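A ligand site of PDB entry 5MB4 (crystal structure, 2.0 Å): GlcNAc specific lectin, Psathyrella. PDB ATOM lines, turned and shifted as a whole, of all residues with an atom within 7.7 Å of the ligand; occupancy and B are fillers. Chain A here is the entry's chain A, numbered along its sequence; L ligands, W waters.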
ATOM      1  N   ASN A  45     -12.066  19.897 -21.566  1.00  0.00           N
ATOM      2  CA  ASN A  45     -10.987  20.138 -22.507  1.00  0.00           C
ATOM      3  C   ASN A  45     -10.262  21.426 -22.137  1.00  0.00           C
ATOM      4  O   ASN A  45     -10.186  22.351 -22.923  1.00  0.00           O
ATOM      5  CB  ASN A  45     -11.557  20.101 -23.954  1.00  0.00           C
ATOM      6  CG  ASN A  45     -10.460  20.149 -25.044  1.00  0.00           C
ATOM      7  OD1 ASN A  45     -10.708  20.767 -26.080  1.00  0.00           O
ATOM      8  ND2 ASN A  45      -9.299  19.513 -24.839  1.00  0.00           N
ATOM      9  N   ASN A  46      -9.755  21.469 -20.896  1.00  0.00           N
ATOM     10  CA  ASN A  46      -9.091  22.635 -20.288  1.00  0.00           C
ATOM     11  C   ASN A  46      -8.340  22.203 -19.031  1.00  0.00           C
ATOM     12  O   ASN A  46      -8.355  21.031 -18.706  1.00  0.00           O
ATOM     13  CB  ASN A  46     -10.073  23.753 -19.936  1.00  0.00           C
ATOM     14  CG  ASN A  46      -9.510  25.117 -20.270  1.00  0.00           C
ATOM     15  OD1 ASN A  46      -8.445  25.501 -19.806  1.00  0.00           O
ATOM     16  ND2 ASN A  46     -10.254  25.850 -21.092  1.00  0.00           N
ATOM     17  N   PHE A  47      -7.667  23.124 -18.382  1.00  0.00           N
ATOM     18  CA  PHE A  47      -6.852  22.807 -17.199  1.00  0.00           C
ATOM     19  C   PHE A  47      -5.700  21.835 -17.438  1.00  0.00           C
ATOM     20  O   PHE A  47      -5.183  21.237 -16.474  1.00  0.00           O
ATOM     21  CB  PHE A  47      -7.716  22.335 -16.030  1.00  0.00           C
ATOM     22  CG  PHE A  47      -8.799  23.309 -15.641  1.00  0.00           C
ATOM     23  CD1 PHE A  47      -8.510  24.438 -14.876  1.00  0.00           C
ATOM     24  CD2 PHE A  47     -10.132  23.127 -16.041  1.00  0.00           C
ATOM     25  CE1 PHE A  47      -9.522  25.308 -14.500  1.00  0.00           C
ATOM     26  CE2 PHE A  47     -11.140  24.005 -15.675  1.00  0.00           C
ATOM     27  CZ  PHE A  47     -10.825  25.103 -14.896  1.00  0.00           C
ATOM     28  N   GLY A  48      -5.258  21.748 -18.704  1.00  0.00           N
ATOM     29  CA  GLY A  48      -4.214  20.839 -19.116  1.00  0.00           C
ATOM     30  C   GLY A  48      -2.976  21.487 -19.723  1.00  0.00           C
ATOM     31  O   GLY A  48      -3.070  22.528 -20.340  1.00  0.00           O
ATOM     32  N   ALA A  51      -3.948  21.927 -23.073  1.00  0.00           N
ATOM     33  CA  ALA A  51      -5.340  22.290 -23.166  1.00  0.00           C
ATOM     34  C   ALA A  51      -5.497  23.485 -22.232  1.00  0.00           C
ATOM     35  O   ALA A  51      -5.948  23.361 -21.063  1.00  0.00           O
ATOM     36  CB  ALA A  51      -6.243  21.124 -22.771  1.00  0.00           C
ATOM     37  N   GLY A  52      -4.991  24.606 -22.753  1.00  0.00           N
ATOM     38  CA  GLY A  52      -5.046  25.878 -22.120  1.00  0.00           C
ATOM     39  C   GLY A  52      -3.725  26.328 -21.587  1.00  0.00           C
ATOM     40  O   GLY A  52      -3.671  27.391 -20.966  1.00  0.00           O
ATOM     41  N   GLY A  53      -2.673  25.571 -21.815  1.00  0.00           N
ATOM     42  CA  GLY A  53      -1.317  26.003 -21.403  1.00  0.00           C
ATOM     43  C   GLY A  53      -1.020  25.956 -19.887  1.00  0.00           C
ATOM     44  O   GLY A  53      -0.193  26.722 -19.377  1.00  0.00           O
ATOM     45  N   TRP A  54      -1.640  25.015 -19.181  1.00  0.00           N
ATOM     46  CA  TRP A  54      -1.511  24.938 -17.726  1.00  0.00           C
ATOM     47  C   TRP A  54      -0.150  24.342 -17.392  1.00  0.00           C
ATOM     48  O   TRP A  54       0.287  23.418 -18.057  1.00  0.00           O
ATOM     49  CB  TRP A  54      -2.734  24.192 -17.085  1.00  0.00           C
ATOM     50  CG  TRP A  54      -3.970  24.999 -17.190  1.00  0.00           C
ATOM     51  CD1 TRP A  54      -4.706  25.254 -18.334  1.00  0.00           C
ATOM     52  CD2 TRP A  54      -4.571  25.777 -16.162  1.00  0.00           C
ATOM     53  NE1 TRP A  54      -5.747  26.082 -18.057  1.00  0.00           N
ATOM     54  CE2 TRP A  54      -5.682  26.439 -16.727  1.00  0.00           C
ATOM     55  CE3 TRP A  54      -4.305  25.949 -14.809  1.00  0.00           C
ATOM     56  CZ2 TRP A  54      -6.498  27.285 -16.004  1.00  0.00           C
ATOM     57  CZ3 TRP A  54      -5.148  26.799 -14.073  1.00  0.00           C
ATOM     58  CH2 TRP A  54      -6.226  27.454 -14.687  1.00  0.00           C
ATOM     59  N   ARG A  55       0.551  24.911 -16.402  1.00  0.00           N
ATOM     60  CA  ARG A  55       1.880  24.499 -16.017  1.00  0.00           C
ATOM     61  C   ARG A  55       2.006  24.356 -14.512  1.00  0.00           C
ATOM     62  O   ARG A  55       1.569  25.214 -13.719  1.00  0.00           O
ATOM     63  CB  ARG A  55       2.937  25.503 -16.463  1.00  0.00           C
ATOM     64  CG  ARG A  55       3.003  25.715 -17.952  1.00  0.00           C
ATOM     65  CD  ARG A  55       3.745  24.602 -18.638  1.00  0.00           C
ATOM     66  NE  ARG A  55       3.809  24.830 -20.087  1.00  0.00           N
ATOM     67  CZ  ARG A  55       2.864  24.536 -20.957  1.00  0.00           C
ATOM     68  NH1 ARG A  55       1.722  24.031 -20.586  1.00  0.00           N
ATOM     69  NH2 ARG A  55       3.079  24.760 -22.247  1.00  0.00           N
ATOM     70  N   LYS A  58       3.661  27.294 -12.855  1.00  0.00           N
ATOM     71  CA  LYS A  58       3.025  28.610 -12.783  1.00  0.00           C
ATOM     72  C   LYS A  58       1.583  28.650 -12.285  1.00  0.00           C
ATOM     73  O   LYS A  58       1.071  29.763 -11.973  1.00  0.00           O
ATOM     74  CB  LYS A  58       3.050  29.238 -14.186  1.00  0.00           C
ATOM     75  CG  LYS A  58       4.436  29.451 -14.794  1.00  0.00           C
ATOM     76  CD  LYS A  58       4.269  29.955 -16.229  1.00  0.00           C
ATOM     77  CE  LYS A  58       4.101  31.471 -16.274  1.00  0.00           C
ATOM     78  NZ  LYS A  58       3.643  32.075 -17.573  1.00  0.00           N
ATOM     79  N   HIS A  59       0.885  27.514 -12.279  1.00  0.00           N
ATOM     80  CA  HIS A  59      -0.516  27.453 -11.981  1.00  0.00           C
ATOM     81  C   HIS A  59      -0.818  26.389 -10.916  1.00  0.00           C
ATOM     82  O   HIS A  59       0.030  25.535 -10.628  1.00  0.00           O
ATOM     83  CB  HIS A  59      -1.289  27.188 -13.272  1.00  0.00           C
ATOM     84  CG  HIS A  59      -0.867  28.059 -14.417  1.00  0.00           C
ATOM     85  ND1 HIS A  59      -0.453  27.541 -15.622  1.00  0.00           N
ATOM     86  CD2 HIS A  59      -0.772  29.403 -14.563  1.00  0.00           C
ATOM     87  CE1 HIS A  59      -0.171  28.507 -16.471  1.00  0.00           C
ATOM     88  NE2 HIS A  59      -0.354  29.658 -15.851  1.00  0.00           N
ATOM     89  N   ARG A  61      -4.071  23.805  -9.637  1.00  0.00           N
ATOM     90  CA  ARG A  61      -5.309  23.141  -9.983  1.00  0.00           C
ATOM     91  C   ARG A  61      -5.795  22.286  -8.796  1.00  0.00           C
ATOM     92  O   ARG A  61      -5.033  21.460  -8.241  1.00  0.00           O
ATOM     93  CB  ARG A  61      -5.062  22.317 -11.234  1.00  0.00           C
ATOM     94  CG  ARG A  61      -4.959  23.202 -12.477  1.00  0.00           C
ATOM     95  CD  ARG A  61      -4.300  22.487 -13.658  1.00  0.00           C
ATOM     96  NE  ARG A  61      -2.882  22.302 -13.438  1.00  0.00           N
ATOM     97  CZ  ARG A  61      -2.081  21.693 -14.314  1.00  0.00           C
ATOM     98  NH1 ARG A  61      -2.573  21.191 -15.439  1.00  0.00           N
ATOM     99  NH2 ARG A  61      -0.800  21.556 -14.046  1.00  0.00           N
ATOM    100  N   GLY A  76      -9.050  26.354 -11.100  1.00  0.00           N
ATOM    101  CA  GLY A  76      -7.665  26.595 -11.566  1.00  0.00           C
ATOM    102  C   GLY A  76      -7.227  28.017 -11.319  1.00  0.00           C
ATOM    103  O   GLY A  76      -7.919  28.928 -11.734  1.00  0.00           O
ATOM    104  N   PHE A  77      -6.075  28.180 -10.671  1.00  0.00           N
ATOM    105  CA  PHE A  77      -5.420  29.499 -10.565  1.00  0.00           C
ATOM    106  C   PHE A  77      -4.476  29.624 -11.760  1.00  0.00           C
ATOM    107  O   PHE A  77      -3.370  29.088 -11.761  1.00  0.00           O
ATOM    108  CB  PHE A  77      -4.632  29.604  -9.268  1.00  0.00           C
ATOM    109  CG  PHE A  77      -5.474  29.471  -8.039  1.00  0.00           C
ATOM    110  CD1 PHE A  77      -5.869  28.228  -7.574  1.00  0.00           C
ATOM    111  CD2 PHE A  77      -5.927  30.587  -7.394  1.00  0.00           C
ATOM    112  CE1 PHE A  77      -6.661  28.099  -6.443  1.00  0.00           C
ATOM    113  CE2 PHE A  77      -6.723  30.460  -6.272  1.00  0.00           C
ATOM    114  CZ  PHE A  77      -7.078  29.203  -5.783  1.00  0.00           C
ATOM    115  N   GLY A  78      -4.953  30.320 -12.791  1.00  0.00           N
ATOM    116  CA  GLY A  78      -4.289  30.316 -14.084  1.00  0.00           C
ATOM    117  C   GLY A  78      -3.398  31.536 -14.303  1.00  0.00           C
ATOM    118  O   GLY A  78      -2.784  32.074 -13.353  1.00  0.00           O
ATOM    119  N   GLU A  79      -3.308  31.941 -15.570  1.00  0.00           N
ATOM    120  CA  GLU A  79      -2.365  33.021 -15.950  1.00  0.00           C
ATOM    121  C   GLU A  79      -2.873  34.424 -15.527  1.00  0.00           C
ATOM    122  O   GLU A  79      -2.110  35.249 -15.008  1.00  0.00           O
ATOM    123  CB  GLU A  79      -2.130  32.948 -17.484  1.00  0.00           C
ATOM    124  CG  GLU A  79      -0.922  33.694 -18.019  1.00  0.00           C
ATOM    125  CD  GLU A  79       0.433  33.156 -17.532  1.00  0.00           C
ATOM    126  OE1 GLU A  79       0.494  32.097 -16.895  1.00  0.00           O
ATOM    127  OE2 GLU A  79       1.454  33.834 -17.785  1.00  0.00           O
ATOM    128  N   ASP A  80      -4.158  34.655 -15.735  1.00  0.00           N
ATOM    129  CA  ASP A  80      -4.798  35.950 -15.577  1.00  0.00           C
ATOM    130  C   ASP A  80      -5.940  36.009 -14.573  1.00  0.00           C
ATOM    131  O   ASP A  80      -6.537  37.088 -14.414  1.00  0.00           O
ATOM    132  CB  ASP A  80      -5.313  36.382 -16.954  1.00  0.00           C
ATOM    133  CG  ASP A  80      -4.175  36.564 -17.936  1.00  0.00           C
ATOM    134  OD1 ASP A  80      -3.209  37.290 -17.605  1.00  0.00           O
ATOM    135  OD2 ASP A  80      -4.200  35.916 -19.004  1.00  0.00           O
ATOM    136  N   GLY A  81      -6.219  34.900 -13.887  1.00  0.00           N
ATOM    137  CA  GLY A  81      -7.357  34.830 -12.998  1.00  0.00           C
ATOM    138  C   GLY A  81      -7.713  33.399 -12.567  1.00  0.00           C
ATOM    139  O   GLY A  81      -7.040  32.442 -12.948  1.00  0.00           O
ATOM    140  N   VAL A  82      -8.774  33.296 -11.774  1.00  0.00           N
ATOM    141  CA  VAL A  82      -9.225  32.017 -11.229  1.00  0.00           C
ATOM    142  C   VAL A  82     -10.306  31.529 -12.150  1.00  0.00           C
ATOM    143  O   VAL A  82     -11.209  32.275 -12.467  1.00  0.00           O
ATOM    144  CB  VAL A  82      -9.765  32.167  -9.804  1.00  0.00           C
ATOM    145  CG1 VAL A  82     -10.193  30.827  -9.240  1.00  0.00           C
ATOM    146  CG2 VAL A  82      -8.692  32.764  -8.905  1.00  0.00           C
ATOM    147  N   TRP A  83     -10.190  30.273 -12.571  1.00  0.00           N
ATOM    148  CA  TRP A  83     -11.086  29.652 -13.538  1.00  0.00           C
ATOM    149  C   TRP A  83     -11.801  28.478 -12.888  1.00  0.00           C
ATOM    150  O   TRP A  83     -11.149  27.643 -12.246  1.00  0.00           O
ATOM    151  CB  TRP A  83     -10.292  29.133 -14.722  1.00  0.00           C
ATOM    152  CG  TRP A  83      -9.755  30.215 -15.624  1.00  0.00           C
ATOM    153  CD1 TRP A  83      -8.547  30.862 -15.527  1.00  0.00           C
ATOM    154  CD2 TRP A  83     -10.388  30.742 -16.781  1.00  0.00           C
ATOM    155  NE1 TRP A  83      -8.403  31.759 -16.550  1.00  0.00           N
ATOM    156  CE2 TRP A  83      -9.534  31.722 -17.317  1.00  0.00           C
ATOM    157  CE3 TRP A  83     -11.606  30.483 -17.417  1.00  0.00           C
ATOM    158  CZ2 TRP A  83      -9.832  32.426 -18.477  1.00  0.00           C
ATOM    159  CZ3 TRP A  83     -11.946  31.211 -18.574  1.00  0.00           C
ATOM    160  CH2 TRP A  83     -11.038  32.154 -19.099  1.00  0.00           C
ATOM    161  N   PRO A  96     -16.543  25.422 -21.720  1.00  0.00           N
ATOM    162  CA  PRO A  96     -15.324  25.850 -21.039  1.00  0.00           C
ATOM    163  C   PRO A  96     -15.545  26.374 -19.623  1.00  0.00           C
ATOM    164  O   PRO A  96     -16.681  26.738 -19.299  1.00  0.00           O
ATOM    165  CB  PRO A  96     -14.818  26.993 -21.946  1.00  0.00           C
ATOM    166  CG  PRO A  96     -16.097  27.612 -22.452  1.00  0.00           C
ATOM    167  CD  PRO A  96     -16.997  26.435 -22.697  1.00  0.00           C
ATOM    168  N   PRO A  97     -14.466  26.414 -18.800  1.00  0.00           N
ATOM    169  CA  PRO A  97     -14.691  26.991 -17.513  1.00  0.00           C
ATOM    170  C   PRO A  97     -14.934  28.490 -17.610  1.00  0.00           C
ATOM    171  O   PRO A  97     -14.756  29.107 -18.645  1.00  0.00           O
ATOM    172  CB  PRO A  97     -13.397  26.724 -16.761  1.00  0.00           C
ATOM    173  CG  PRO A  97     -12.356  26.690 -17.805  1.00  0.00           C
ATOM    174  CD  PRO A  97     -13.035  26.093 -19.012  1.00  0.00           C
ATOM    175  N   HIS A  99     -14.155  32.340 -15.846  1.00  0.00           N
ATOM    176  CA  HIS A  99     -13.169  33.105 -15.078  1.00  0.00           C
ATOM    177  C   HIS A  99     -13.921  33.951 -14.058  1.00  0.00           C
ATOM    178  O   HIS A  99     -14.620  34.854 -14.417  1.00  0.00           O
ATOM    179  CB  HIS A  99     -12.355  33.908 -16.081  1.00  0.00           C
ATOM    180  CG  HIS A  99     -11.338  34.805 -15.480  1.00  0.00           C
ATOM    181  ND1 HIS A  99     -10.334  35.371 -16.224  1.00  0.00           N
ATOM    182  CD2 HIS A  99     -11.217  35.304 -14.235  1.00  0.00           C
ATOM    183  CE1 HIS A  99      -9.633  36.184 -15.459  1.00  0.00           C
ATOM    184  NE2 HIS A  99     -10.147  36.144 -14.252  1.00  0.00           N
ATOM    185  N   SER A 105      -3.360  34.999  -9.423  1.00  0.00           N
ATOM    186  CA  SER A 105      -2.823  34.419 -10.662  1.00  0.00           C
ATOM    187  C   SER A 105      -1.482  35.020 -11.012  1.00  0.00           C
ATOM    188  O   SER A 105      -1.056  36.004 -10.376  1.00  0.00           O
ATOM    189  CB  SER A 105      -3.816  34.581 -11.801  1.00  0.00           C
ATOM    190  OG  SER A 105      -3.778  35.925 -12.258  1.00  0.00           O
HETATM  191  C1  LIG L   1      -5.842  30.845 -20.762  1.00  0.00           C
HETATM  192  C2  LIG L   1      -6.216  29.788 -19.720  1.00  0.00           C
HETATM  193  C3  LIG L   1      -7.214  28.801 -20.297  1.00  0.00           C
HETATM  194  C4  LIG L   1      -8.396  29.523 -20.939  1.00  0.00           C
HETATM  195  C5  LIG L   1      -7.901  30.641 -21.859  1.00  0.00           C
HETATM  196  C6  LIG L   1      -9.079  31.482 -22.381  1.00  0.00           C
HETATM  197  C7  LIG L   1      -4.420  29.491 -18.157  1.00  0.00           C
HETATM  198  C8  LIG L   1      -3.222  28.679 -17.791  1.00  0.00           C
HETATM  199  N1  LIG L   1      -5.058  29.101 -19.248  1.00  0.00           N
HETATM  200  O1  LIG L   1      -5.127  31.846 -20.119  1.00  0.00           O
HETATM  201  O2  LIG L   1      -7.711  27.957 -19.292  1.00  0.00           O
HETATM  202  O3  LIG L   1      -9.107  28.597 -21.719  1.00  0.00           O
HETATM  203  O4  LIG L   1      -7.008  31.505 -21.192  1.00  0.00           O
HETATM  204  O5  LIG L   1      -8.605  32.411 -23.331  1.00  0.00           O
HETATM  205  O6  LIG L   1      -4.742  30.456 -17.462  1.00  0.00           O
HETATM  206  O   HOH W   1      -6.067  32.912 -17.332  1.00  0.00           O
HETATM  207  O   HOH W   2      -7.951  27.174 -23.889  1.00  0.00           O
HETATM  208  O   HOH W   3      -6.622  34.354 -19.524  1.00  0.00           O
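OD1 of Asn 46 lies within hydrogen-bond range of O2 of the ligand, 2.6 Å away.
O of Gly 52 lies within hydrogen-bond range of N1 of the ligand (2.8 Å).
The backbone NH of Glu 79 sits at hydrogen-bond distance from an oxygen (O6) of the ligand (2.8 Å).
An oxygen (O2) of the ligand lies within hydrogen-bond range of the indole nitrogen (NE1) of Trp 54, 3.0 Å away.
ND1 of His 59 is in hydrogen-bond range of N of Arg 55 (2.9 Å).
N of Trp 54 is in hydrogen-bond range of O of Gly 48, at 3.1 Å.
The backbone carbonyl oxygen (O) of Trp 83 lies within hydrogen-bond range of the backbone NH (N) of Gly 76, at 2.7 Å.
OE1 of Glu 79 is in hydrogen-bond range of NE2 of His 59 (2.8 Å).
The side-chain carboxylate of Glu 79 is in salt-bridge range of the side-chain amino group of Lys 58 (2.8 Å).
The backbone carbonyl oxygen (O) of Glu 79 sits at hydrogen-bond distance from the side-chain hydroxyl (OG) of Ser 105.
NE1 of Trp 54 is in hydrogen-bond range of OD1 of Asn 46, at 3.3 Å.
The backbone NH of Gly 53 is in hydrogen-bond range of the backbone carbonyl oxygen of Gly 48 (3.4 Å).
Residues that only touch the ligand: Gly 53 (3.9 Å), His 59 (3.3 Å), Gly 78 (3.4 Å) and Trp 83 (3.9 Å).
Hydrophobic or aromatic side chains that line the ligand: Trp 54, His 59 and Trp 83.
Along chain A the residues within 4 Å of the ligand span positions 46 to 83.
Water W3 lies within hydrogen-bond range of OD2 of Asp 80 (2.9 Å) and O1 of the ligand (3.0 Å).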
